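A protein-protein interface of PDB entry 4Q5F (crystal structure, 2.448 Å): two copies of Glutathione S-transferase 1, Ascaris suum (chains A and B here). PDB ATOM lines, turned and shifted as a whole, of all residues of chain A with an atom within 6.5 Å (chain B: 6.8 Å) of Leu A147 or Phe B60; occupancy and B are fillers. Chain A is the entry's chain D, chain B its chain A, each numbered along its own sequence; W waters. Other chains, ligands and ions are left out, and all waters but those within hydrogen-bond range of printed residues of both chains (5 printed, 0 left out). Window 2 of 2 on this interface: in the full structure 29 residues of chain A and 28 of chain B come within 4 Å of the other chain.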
ATOM      1  N   GLN A  99      28.611  -9.076  12.625  1.00  0.00           N
ATOM      2  CA  GLN A  99      27.163  -9.173  12.764  1.00  0.00           C
ATOM      3  C   GLN A  99      26.537  -7.781  12.756  1.00  0.00           C
ATOM      4  O   GLN A  99      25.437  -7.592  12.235  1.00  0.00           O
ATOM      5  CB  GLN A  99      26.785  -9.913  14.049  1.00  0.00           C
ATOM      6  CG  GLN A  99      27.148 -11.393  14.050  1.00  0.00           C
ATOM      7  CD  GLN A  99      26.400 -12.189  12.995  1.00  0.00           C
ATOM      8  OE1 GLN A  99      25.319 -11.800  12.550  1.00  0.00           O
ATOM      9  NE2 GLN A  99      26.979 -13.310  12.586  1.00  0.00           N
ATOM     10  N   SER A 102      26.556  -6.768   9.293  1.00  0.00           N
ATOM     11  CA  SER A 102      25.596  -7.575   8.555  1.00  0.00           C
ATOM     12  C   SER A 102      24.195  -6.980   8.625  1.00  0.00           C
ATOM     13  O   SER A 102      23.535  -6.809   7.602  1.00  0.00           O
ATOM     14  CB  SER A 102      25.582  -9.007   9.093  1.00  0.00           C
ATOM     15  OG  SER A 102      24.828  -9.860   8.248  1.00  0.00           O
ATOM     16  N   ILE A 103      23.739  -6.657   9.830  1.00  0.00           N
ATOM     17  CA  ILE A 103      22.382  -6.152   9.995  1.00  0.00           C
ATOM     18  C   ILE A 103      22.219  -4.770   9.365  1.00  0.00           C
ATOM     19  O   ILE A 103      21.146  -4.435   8.866  1.00  0.00           O
ATOM     20  CB  ILE A 103      21.955  -6.112  11.484  1.00  0.00           C
ATOM     21  CG1 ILE A 103      20.483  -5.696  11.619  1.00  0.00           C
ATOM     22  CG2 ILE A 103      22.844  -5.172  12.282  1.00  0.00           C
ATOM     23  CD1 ILE A 103      19.499  -6.649  10.957  1.00  0.00           C
ATOM     24  N   PHE A 104      23.279  -3.968   9.382  1.00  0.00           N
ATOM     25  CA  PHE A 104      23.204  -2.637   8.791  1.00  0.00           C
ATOM     26  C   PHE A 104      23.171  -2.711   7.267  1.00  0.00           C
ATOM     27  O   PHE A 104      22.516  -1.896   6.620  1.00  0.00           O
ATOM     28  CB  PHE A 104      24.361  -1.746   9.245  1.00  0.00           C
ATOM     29  CG  PHE A 104      24.244  -0.331   8.758  1.00  0.00           C
ATOM     30  CD1 PHE A 104      23.342   0.540   9.344  1.00  0.00           C
ATOM     31  CD2 PHE A 104      25.020   0.125   7.705  1.00  0.00           C
ATOM     32  CE1 PHE A 104      23.221   1.842   8.896  1.00  0.00           C
ATOM     33  CE2 PHE A 104      24.904   1.428   7.254  1.00  0.00           C
ATOM     34  CZ  PHE A 104      24.004   2.286   7.849  1.00  0.00           C
ATOM     35  N   ASP A 105      23.876  -3.685   6.699  1.00  0.00           N
ATOM     36  CA  ASP A 105      23.845  -3.901   5.256  1.00  0.00           C
ATOM     37  C   ASP A 105      22.445  -4.307   4.802  1.00  0.00           C
ATOM     38  O   ASP A 105      22.004  -3.936   3.714  1.00  0.00           O
ATOM     39  CB  ASP A 105      24.853  -4.975   4.839  1.00  0.00           C
ATOM     40  CG  ASP A 105      26.265  -4.434   4.683  1.00  0.00           C
ATOM     41  OD1 ASP A 105      26.465  -3.206   4.804  1.00  0.00           O
ATOM     42  OD2 ASP A 105      27.180  -5.244   4.425  1.00  0.00           O
ATOM     43  N   GLN A 106      21.749  -5.078   5.630  1.00  0.00           N
ATOM     44  CA  GLN A 106      20.383  -5.476   5.312  1.00  0.00           C
ATOM     45  C   GLN A 106      19.469  -4.260   5.403  1.00  0.00           C
ATOM     46  O   GLN A 106      18.561  -4.087   4.588  1.00  0.00           O
ATOM     47  CB  GLN A 106      19.892  -6.577   6.254  1.00  0.00           C
ATOM     48  CG  GLN A 106      18.497  -7.095   5.920  1.00  0.00           C
ATOM     49  CD  GLN A 106      18.414  -7.697   4.529  1.00  0.00           C
ATOM     50  OE1 GLN A 106      19.401  -8.208   4.002  1.00  0.00           O
ATOM     51  NE2 GLN A 106      17.231  -7.637   3.925  1.00  0.00           N
ATOM     52  N   ASP A 142       7.034  -4.673   3.997  1.00  0.00           N
ATOM     53  CA  ASP A 142       6.555  -5.999   4.363  1.00  0.00           C
ATOM     54  C   ASP A 142       7.634  -7.070   4.232  1.00  0.00           C
ATOM     55  O   ASP A 142       7.618  -8.057   4.967  1.00  0.00           O
ATOM     56  CB  ASP A 142       5.335  -6.374   3.520  1.00  0.00           C
ATOM     57  CG  ASP A 142       4.110  -5.538   3.860  1.00  0.00           C
ATOM     58  OD1 ASP A 142       4.263  -4.506   4.549  1.00  0.00           O
ATOM     59  OD2 ASP A 142       2.997  -5.905   3.430  1.00  0.00           O
ATOM     60  N   LYS A 143       8.568  -6.884   3.305  1.00  0.00           N
ATOM     61  CA  LYS A 143       9.656  -7.845   3.138  1.00  0.00           C
ATOM     62  C   LYS A 143      10.736  -7.674   4.202  1.00  0.00           C
ATOM     63  O   LYS A 143      11.207  -8.652   4.780  1.00  0.00           O
ATOM     64  CB  LYS A 143      10.300  -7.721   1.754  1.00  0.00           C
ATOM     65  CG  LYS A 143      11.278  -8.857   1.451  1.00  0.00           C
ATOM     66  CD  LYS A 143      12.176  -8.573   0.256  1.00  0.00           C
ATOM     67  CE  LYS A 143      12.772  -9.869  -0.282  1.00  0.00           C
ATOM     68  NZ  LYS A 143      13.979  -9.648  -1.126  1.00  0.00           N
ATOM     69  N   HIS A 144      11.125  -6.428   4.457  1.00  0.00           N
ATOM     70  CA  HIS A 144      12.342  -6.151   5.218  1.00  0.00           C
ATOM     71  C   HIS A 144      12.159  -6.077   6.733  1.00  0.00           C
ATOM     72  O   HIS A 144      13.017  -6.545   7.482  1.00  0.00           O
ATOM     73  CB  HIS A 144      12.991  -4.866   4.709  1.00  0.00           C
ATOM     74  CG  HIS A 144      13.687  -5.030   3.394  1.00  0.00           C
ATOM     75  ND1 HIS A 144      14.960  -5.547   3.291  1.00  0.00           N
ATOM     76  CD2 HIS A 144      13.284  -4.761   2.131  1.00  0.00           C
ATOM     77  CE1 HIS A 144      15.315  -5.579   2.016  1.00  0.00           C
ATOM     78  NE2 HIS A 144      14.318  -5.111   1.295  1.00  0.00           N
ATOM     79  N   LEU A 145      11.057  -5.488   7.186  1.00  0.00           N
ATOM     80  CA  LEU A 145      10.817  -5.345   8.620  1.00  0.00           C
ATOM     81  C   LEU A 145      10.814  -6.688   9.359  1.00  0.00           C
ATOM     82  O   LEU A 145      11.427  -6.805  10.418  1.00  0.00           O
ATOM     83  CB  LEU A 145       9.515  -4.585   8.886  1.00  0.00           C
ATOM     84  CG  LEU A 145       9.488  -3.106   8.487  1.00  0.00           C
ATOM     85  CD1 LEU A 145       8.180  -2.471   8.932  1.00  0.00           C
ATOM     86  CD2 LEU A 145      10.669  -2.331   9.061  1.00  0.00           C
ATOM     87  N   PRO A 146      10.122  -7.702   8.814  1.00  0.00           N
ATOM     88  CA  PRO A 146      10.197  -9.010   9.478  1.00  0.00           C
ATOM     89  C   PRO A 146      11.627  -9.545   9.590  1.00  0.00           C
ATOM     90  O   PRO A 146      11.950 -10.226  10.562  1.00  0.00           O
ATOM     91  CB  PRO A 146       9.356  -9.928   8.577  1.00  0.00           C
ATOM     92  CG  PRO A 146       8.851  -9.084   7.455  1.00  0.00           C
ATOM     93  CD  PRO A 146       9.052  -7.656   7.805  1.00  0.00           C
ATOM     94  N   LEU A 147      12.470  -9.237   8.609  1.00  0.00           N
ATOM     95  CA  LEU A 147      13.855  -9.699   8.625  1.00  0.00           C
ATOM     96  C   LEU A 147      14.674  -8.972   9.692  1.00  0.00           C
ATOM     97  O   LEU A 147      15.521  -9.575  10.349  1.00  0.00           O
ATOM     98  CB  LEU A 147      14.498  -9.526   7.245  1.00  0.00           C
ATOM     99  CG  LEU A 147      13.813 -10.295   6.111  1.00  0.00           C
ATOM    100  CD1 LEU A 147      14.381  -9.898   4.759  1.00  0.00           C
ATOM    101  CD2 LEU A 147      13.937 -11.798   6.320  1.00  0.00           C
ATOM    102  N   LEU A 148      14.423  -7.677   9.864  1.00  0.00           N
ATOM    103  CA  LEU A 148      15.091  -6.912  10.911  1.00  0.00           C
ATOM    104  C   LEU A 148      14.608  -7.361  12.286  1.00  0.00           C
ATOM    105  O   LEU A 148      15.386  -7.442  13.239  1.00  0.00           O
ATOM    106  CB  LEU A 148      14.832  -5.412  10.741  1.00  0.00           C
ATOM    107  CG  LEU A 148      15.390  -4.709   9.499  1.00  0.00           C
ATOM    108  CD1 LEU A 148      15.133  -3.212   9.594  1.00  0.00           C
ATOM    109  CD2 LEU A 148      16.876  -4.982   9.316  1.00  0.00           C
ATOM    110  N   GLU A 149      13.313  -7.653  12.378  1.00  0.00           N
ATOM    111  CA  GLU A 149      12.698  -8.056  13.635  1.00  0.00           C
ATOM    112  C   GLU A 149      13.139  -9.465  14.015  1.00  0.00           C
ATOM    113  O   GLU A 149      13.345  -9.764  15.192  1.00  0.00           O
ATOM    114  CB  GLU A 149      11.176  -7.992  13.514  1.00  0.00           C
ATOM    115  CG  GLU A 149      10.454  -7.613  14.794  1.00  0.00           C
ATOM    116  CD  GLU A 149       8.991  -7.293  14.552  1.00  0.00           C
ATOM    117  OE1 GLU A 149       8.438  -7.781  13.545  1.00  0.00           O
ATOM    118  OE2 GLU A 149       8.396  -6.546  15.359  1.00  0.00           O
ATOM    119  N   LYS A 150      13.278 -10.327  13.011  1.00  0.00           N
ATOM    120  CA  LYS A 150      13.777 -11.684  13.215  1.00  0.00           C
ATOM    121  C   LYS A 150      15.173 -11.641  13.821  1.00  0.00           C
ATOM    122  O   LYS A 150      15.457 -12.310  14.814  1.00  0.00           O
ATOM    123  CB  LYS A 150      13.815 -12.435  11.881  1.00  0.00           C
ATOM    124  CG  LYS A 150      14.694 -13.684  11.880  1.00  0.00           C
ATOM    125  CD  LYS A 150      14.587 -14.444  10.567  1.00  0.00           C
ATOM    126  CE  LYS A 150      15.597 -15.580  10.504  1.00  0.00           C
ATOM    127  NZ  LYS A 150      15.331 -16.507   9.369  1.00  0.00           N
ATOM    128  N   PHE A 151      16.040 -10.850  13.198  1.00  0.00           N
ATOM    129  CA  PHE A 151      17.418 -10.693  13.638  1.00  0.00           C
ATOM    130  C   PHE A 151      17.465 -10.158  15.064  1.00  0.00           C
ATOM    131  O   PHE A 151      18.265 -10.605  15.885  1.00  0.00           O
ATOM    132  CB  PHE A 151      18.140  -9.722  12.705  1.00  0.00           C
ATOM    133  CG  PHE A 151      19.636  -9.759  12.821  1.00  0.00           C
ATOM    134  CD1 PHE A 151      20.291  -8.995  13.771  1.00  0.00           C
ATOM    135  CD2 PHE A 151      20.387 -10.549  11.969  1.00  0.00           C
ATOM    136  CE1 PHE A 151      21.669  -9.025  13.872  1.00  0.00           C
ATOM    137  CE2 PHE A 151      21.764 -10.581  12.064  1.00  0.00           C
ATOM    138  CZ  PHE A 151      22.405  -9.819  13.016  1.00  0.00           C
ATOM    139  N   LEU A 152      16.595  -9.195  15.345  1.00  0.00           N
ATOM    140  CA  LEU A 152      16.515  -8.582  16.663  1.00  0.00           C
ATOM    141  C   LEU A 152      16.133  -9.607  17.725  1.00  0.00           C
ATOM    142  O   LEU A 152      16.483  -9.461  18.897  1.00  0.00           O
ATOM    143  CB  LEU A 152      15.489  -7.447  16.643  1.00  0.00           C
ATOM    144  CG  LEU A 152      15.205  -6.746  17.972  1.00  0.00           C
ATOM    145  CD1 LEU A 152      16.477  -6.164  18.572  1.00  0.00           C
ATOM    146  CD2 LEU A 152      14.163  -5.658  17.769  1.00  0.00           C
ATOM    147  N   MET A 160      20.360  -5.251  18.248  1.00  0.00           N
ATOM    148  CA  MET A 160      20.561  -6.212  17.171  1.00  0.00           C
ATOM    149  C   MET A 160      21.666  -7.186  17.536  1.00  0.00           C
ATOM    150  O   MET A 160      21.520  -8.395  17.357  1.00  0.00           O
ATOM    151  CB  MET A 160      20.910  -5.491  15.865  1.00  0.00           C
ATOM    152  CG  MET A 160      19.743  -4.741  15.243  1.00  0.00           C
ATOM    153  SD  MET A 160      18.386  -5.843  14.804  1.00  0.00           S
ATOM    154  CE  MET A 160      17.153  -4.665  14.264  1.00  0.00           C
ATOM    155  N   HIS A 190       4.641  -4.394  13.922  1.00  0.00           N
ATOM    156  CA  HIS A 190       5.981  -4.753  14.384  1.00  0.00           C
ATOM    157  C   HIS A 190       6.340  -4.030  15.674  1.00  0.00           C
ATOM    158  O   HIS A 190       7.115  -3.075  15.656  1.00  0.00           O
ATOM    159  CB  HIS A 190       7.012  -4.378  13.323  1.00  0.00           C
ATOM    160  CG  HIS A 190       6.777  -5.023  11.996  1.00  0.00           C
ATOM    161  ND1 HIS A 190       7.301  -6.256  11.664  1.00  0.00           N
ATOM    162  CD2 HIS A 190       6.082  -4.610  10.913  1.00  0.00           C
ATOM    163  CE1 HIS A 190       6.935  -6.572  10.440  1.00  0.00           C
ATOM    164  NE2 HIS A 190       6.191  -5.588   9.956  1.00  0.00           N
ATOM    165  N   LYS B  55      16.433 -21.329   2.120  1.00  0.00           N
ATOM    166  CA  LYS B  55      16.074 -19.910   2.181  1.00  0.00           C
ATOM    167  C   LYS B  55      15.452 -19.455   3.507  1.00  0.00           C
ATOM    168  O   LYS B  55      15.892 -18.459   4.081  1.00  0.00           O
ATOM    169  CB  LYS B  55      15.136 -19.557   1.023  1.00  0.00           C
ATOM    170  CG  LYS B  55      14.775 -18.082   0.925  1.00  0.00           C
ATOM    171  CD  LYS B  55      13.895 -17.821  -0.287  1.00  0.00           C
ATOM    172  CE  LYS B  55      13.303 -16.421  -0.275  1.00  0.00           C
ATOM    173  NZ  LYS B  55      14.261 -15.390  -0.757  1.00  0.00           N
ATOM    174  N   LYS B  57      15.668 -20.780   6.327  1.00  0.00           N
ATOM    175  CA  LYS B  57      16.566 -21.087   7.432  1.00  0.00           C
ATOM    176  C   LYS B  57      17.768 -20.142   7.465  1.00  0.00           C
ATOM    177  O   LYS B  57      18.658 -20.298   8.300  1.00  0.00           O
ATOM    178  CB  LYS B  57      17.036 -22.541   7.329  1.00  0.00           C
ATOM    179  CG  LYS B  57      15.894 -23.535   7.132  1.00  0.00           C
ATOM    180  CD  LYS B  57      16.123 -24.843   7.879  1.00  0.00           C
ATOM    181  CE  LYS B  57      17.130 -25.739   7.173  1.00  0.00           C
ATOM    182  NZ  LYS B  57      16.462 -26.822   6.396  1.00  0.00           N
ATOM    183  N   THR B  58      17.785 -19.164   6.562  1.00  0.00           N
ATOM    184  CA  THR B  58      18.861 -18.174   6.511  1.00  0.00           C
ATOM    185  C   THR B  58      18.432 -16.884   7.209  1.00  0.00           C
ATOM    186  O   THR B  58      17.239 -16.650   7.401  1.00  0.00           O
ATOM    187  CB  THR B  58      19.257 -17.834   5.060  1.00  0.00           C
ATOM    188  OG1 THR B  58      18.195 -17.111   4.428  1.00  0.00           O
ATOM    189  CG2 THR B  58      19.551 -19.095   4.266  1.00  0.00           C
ATOM    190  N   PRO B  59      19.404 -16.038   7.587  1.00  0.00           N
ATOM    191  CA  PRO B  59      19.100 -14.790   8.300  1.00  0.00           C
ATOM    192  C   PRO B  59      18.188 -13.838   7.528  1.00  0.00           C
ATOM    193  O   PRO B  59      17.198 -13.376   8.095  1.00  0.00           O
ATOM    194  CB  PRO B  59      20.481 -14.153   8.497  1.00  0.00           C
ATOM    195  CG  PRO B  59      21.433 -15.290   8.442  1.00  0.00           C
ATOM    196  CD  PRO B  59      20.857 -16.242   7.446  1.00  0.00           C
ATOM    197  N   PHE B  60      18.518 -13.551   6.270  1.00  0.00           N
ATOM    198  CA  PHE B  60      17.778 -12.564   5.479  1.00  0.00           C
ATOM    199  C   PHE B  60      17.149 -13.164   4.222  1.00  0.00           C
ATOM    200  O   PHE B  60      16.633 -12.435   3.374  1.00  0.00           O
ATOM    201  CB  PHE B  60      18.700 -11.410   5.078  1.00  0.00           C
ATOM    202  CG  PHE B  60      19.415 -10.770   6.235  1.00  0.00           C
ATOM    203  CD1 PHE B  60      18.725 -10.388   7.374  1.00  0.00           C
ATOM    204  CD2 PHE B  60      20.782 -10.555   6.183  1.00  0.00           C
ATOM    205  CE1 PHE B  60      19.386  -9.798   8.436  1.00  0.00           C
ATOM    206  CE2 PHE B  60      21.449  -9.968   7.241  1.00  0.00           C
ATOM    207  CZ  PHE B  60      20.750  -9.588   8.368  1.00  0.00           C
ATOM    208  N   GLY B  61      17.197 -14.486   4.094  1.00  0.00           N
ATOM    209  CA  GLY B  61      16.578 -15.152   2.962  1.00  0.00           C
ATOM    210  C   GLY B  61      17.414 -15.107   1.696  1.00  0.00           C
ATOM    211  O   GLY B  61      16.884 -15.288   0.599  1.00  0.00           O
ATOM    212  N   GLN B  62      18.714 -14.864   1.846  1.00  0.00           N
ATOM    213  CA  GLN B  62      19.600 -14.711   0.695  1.00  0.00           C
ATOM    214  C   GLN B  62      21.003 -15.276   0.928  1.00  0.00           C
ATOM    215  O   GLN B  62      21.424 -15.485   2.063  1.00  0.00           O
ATOM    216  CB  GLN B  62      19.710 -13.236   0.292  1.00  0.00           C
ATOM    217  CG  GLN B  62      18.425 -12.625  -0.244  1.00  0.00           C
ATOM    218  CD  GLN B  62      18.642 -11.267  -0.880  1.00  0.00           C
ATOM    219  OE1 GLN B  62      19.196 -10.358  -0.262  1.00  0.00           O
ATOM    220  NE2 GLN B  62      18.207 -11.127  -2.127  1.00  0.00           N
ATOM    221  N   LEU B  63      21.713 -15.516  -0.169  1.00  0.00           N
ATOM    222  CA  LEU B  63      23.115 -15.910  -0.145  1.00  0.00           C
ATOM    223  C   LEU B  63      23.930 -14.716  -0.647  1.00  0.00           C
ATOM    224  O   LEU B  63      23.385 -13.838  -1.316  1.00  0.00           O
ATOM    225  CB  LEU B  63      23.318 -17.141  -1.032  1.00  0.00           C
ATOM    226  CG  LEU B  63      22.469 -18.359  -0.651  1.00  0.00           C
ATOM    227  CD1 LEU B  63      22.709 -19.509  -1.615  1.00  0.00           C
ATOM    228  CD2 LEU B  63      22.744 -18.803   0.781  1.00  0.00           C
ATOM    229  N   LEU B  65      26.370 -16.874   2.380  1.00  0.00           N
ATOM    230  CA  LEU B  65      26.534 -17.022   3.815  1.00  0.00           C
ATOM    231  C   LEU B  65      27.919 -17.580   4.090  1.00  0.00           C
ATOM    232  O   LEU B  65      28.400 -18.458   3.373  1.00  0.00           O
ATOM    233  CB  LEU B  65      25.487 -17.975   4.390  1.00  0.00           C
ATOM    234  CG  LEU B  65      24.023 -17.544   4.293  1.00  0.00           C
ATOM    235  CD1 LEU B  65      23.119 -18.645   4.825  1.00  0.00           C
ATOM    236  CD2 LEU B  65      23.790 -16.249   5.053  1.00  0.00           C
ATOM    237  N   ALA B  74      25.870 -13.360   7.387  1.00  0.00           N
ATOM    238  CA  ALA B  74      25.243 -13.002   6.117  1.00  0.00           C
ATOM    239  C   ALA B  74      25.807 -11.688   5.576  1.00  0.00           C
ATOM    240  O   ALA B  74      26.622 -11.039   6.233  1.00  0.00           O
ATOM    241  CB  ALA B  74      23.732 -12.906   6.284  1.00  0.00           C
ATOM    242  N   GLN B  75      25.370 -11.322   4.371  1.00  0.00           N
ATOM    243  CA  GLN B  75      25.751 -10.072   3.701  1.00  0.00           C
ATOM    244  C   GLN B  75      27.193 -10.082   3.197  1.00  0.00           C
ATOM    245  O   GLN B  75      28.143 -10.086   3.980  1.00  0.00           O
ATOM    246  CB  GLN B  75      25.486  -8.850   4.591  1.00  0.00           C
ATOM    247  CG  GLN B  75      24.009  -8.584   4.834  1.00  0.00           C
ATOM    248  CD  GLN B  75      23.316  -7.995   3.622  1.00  0.00           C
ATOM    249  OE1 GLN B  75      23.959  -7.647   2.632  1.00  0.00           O
ATOM    250  NE2 GLN B  75      21.994  -7.877   3.696  1.00  0.00           N
HETATM  251  O   HOH W   1      26.829  -6.540   1.777  1.00  0.00           O
HETATM  252  O   HOH W   2      20.278  -9.926   1.953  1.00  0.00           O
HETATM  253  O   HOH W   3      24.451 -12.446   9.708  1.00  0.00           O
HETATM  254  O   HOH W   4      14.924 -12.365  -2.119  1.00  0.00           O
HETATM  255  O   HOH W   5      16.649 -11.779  10.285  1.00  0.00           O
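The side-chain amide nitrogen (NE2) of Gln B75 sits at hydrogen-bond distance from the side-chain amide oxygen (OE1) of Gln A106, 2.6 Å away.
NZ of Lys A150 sits at hydrogen-bond distance from O of Thr B58, 2.7 Å away.
The backbone carbonyl oxygen of Ala B74 is in hydrogen-bond range of the side-chain hydroxyl of Ser A102 (2.9 Å).
OG1 of Thr B58 lies within hydrogen-bond range of N of Gln B62, 3.5 Å away.
ND1 of His A144 sits at hydrogen-bond distance from NE2 of Gln A106 (3.2 Å).
OG1 of Thr B58 sits at hydrogen-bond distance from N of Gly B61, at 2.8 Å.
OG1 of Thr B58 lies within hydrogen-bond range of O of Lys B55 (2.7 Å).
Among the printed residues, pairs that only touch across the chains: Ser A102 with Gln B75, Gln A106 with Phe B60, Ser A102 with Phe B60, Asp A105 with Gln B75, Lys A150 with Pro B59, Leu A147 with Phe B60 and Phe A151 with Phe B60.
Phe B60 touches just these residues of chain A: Ser A102, Gln A106, Leu A147 and Phe A151.
Of the printed residues of chain A, Gln B75 touches Ser A102 (3.3 Å), Asp A105 (3.6 Å) and Gln A106 (2.6 Å).
Of the printed residues of chain B, Ser A102 touches Phe B60 (3.5 Å), Ala B74 (2.9 Å) and Gln B75 (3.3 Å).
Printed residues of chain A within 4 Å of Ala B74: Ser A102 (2.9 Å).
Of the printed residues of chain B, Asp A105 touches Gln B75.
Printed residues of chain A within 4 Å of Pro B59: Lys A150.
The nearest printed residue of chain B that does not touch Lys A150 is Lys B57 (4.8 Å).
Hydrophobic or aromatic side chains of chain B that line the printed part of chain A: Phe B60 and Ala B74.
Printed residues of chain A that touch a printed residue of chain B: Ser A102, Asp A105, Gln A106, Leu A147, Lys A150 and Phe A151.
Hydrophobic or aromatic side chains of chain A that line the printed part of chain B: Leu A147 and Phe A151.
Among the printed residues, no Asp or Glu carboxylate lies within 4 Å of a Lys or Arg side-chain nitrogen of the other chain.
No position is printed for both chains.
Of the 10 pairs that touch across the chains among the printed residues, none has its exchanged pair printed and touching as well.
Water W5 lies within hydrogen-bond range of the backbone carbonyl oxygen of Leu A147 (2.5 Å), the backbone carbonyl oxygen of Pro B59 (2.8 Å) and the backbone NH of Phe A151 (3.1 Å).
Water W2 lies within hydrogen-bond range of OE1 of Gln B62 (2.5 Å), OE1 of Gln A106 (2.8 Å) and NE2 of Gln B75 (3.2 Å).
Water W3 lies within hydrogen-bond range of N of Ala B74 (2.9 Å), OG of Ser A102 (3.0 Å) and OE1 of Gln A99 (3.0 Å).
Water W1 bridges OD2 of Asp A105 (3.0 Å) and OE1 of Gln B75 (3.2 Å).
Water W4 lies within hydrogen-bond range of NZ of Lys A143 and NZ of Lys B55.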
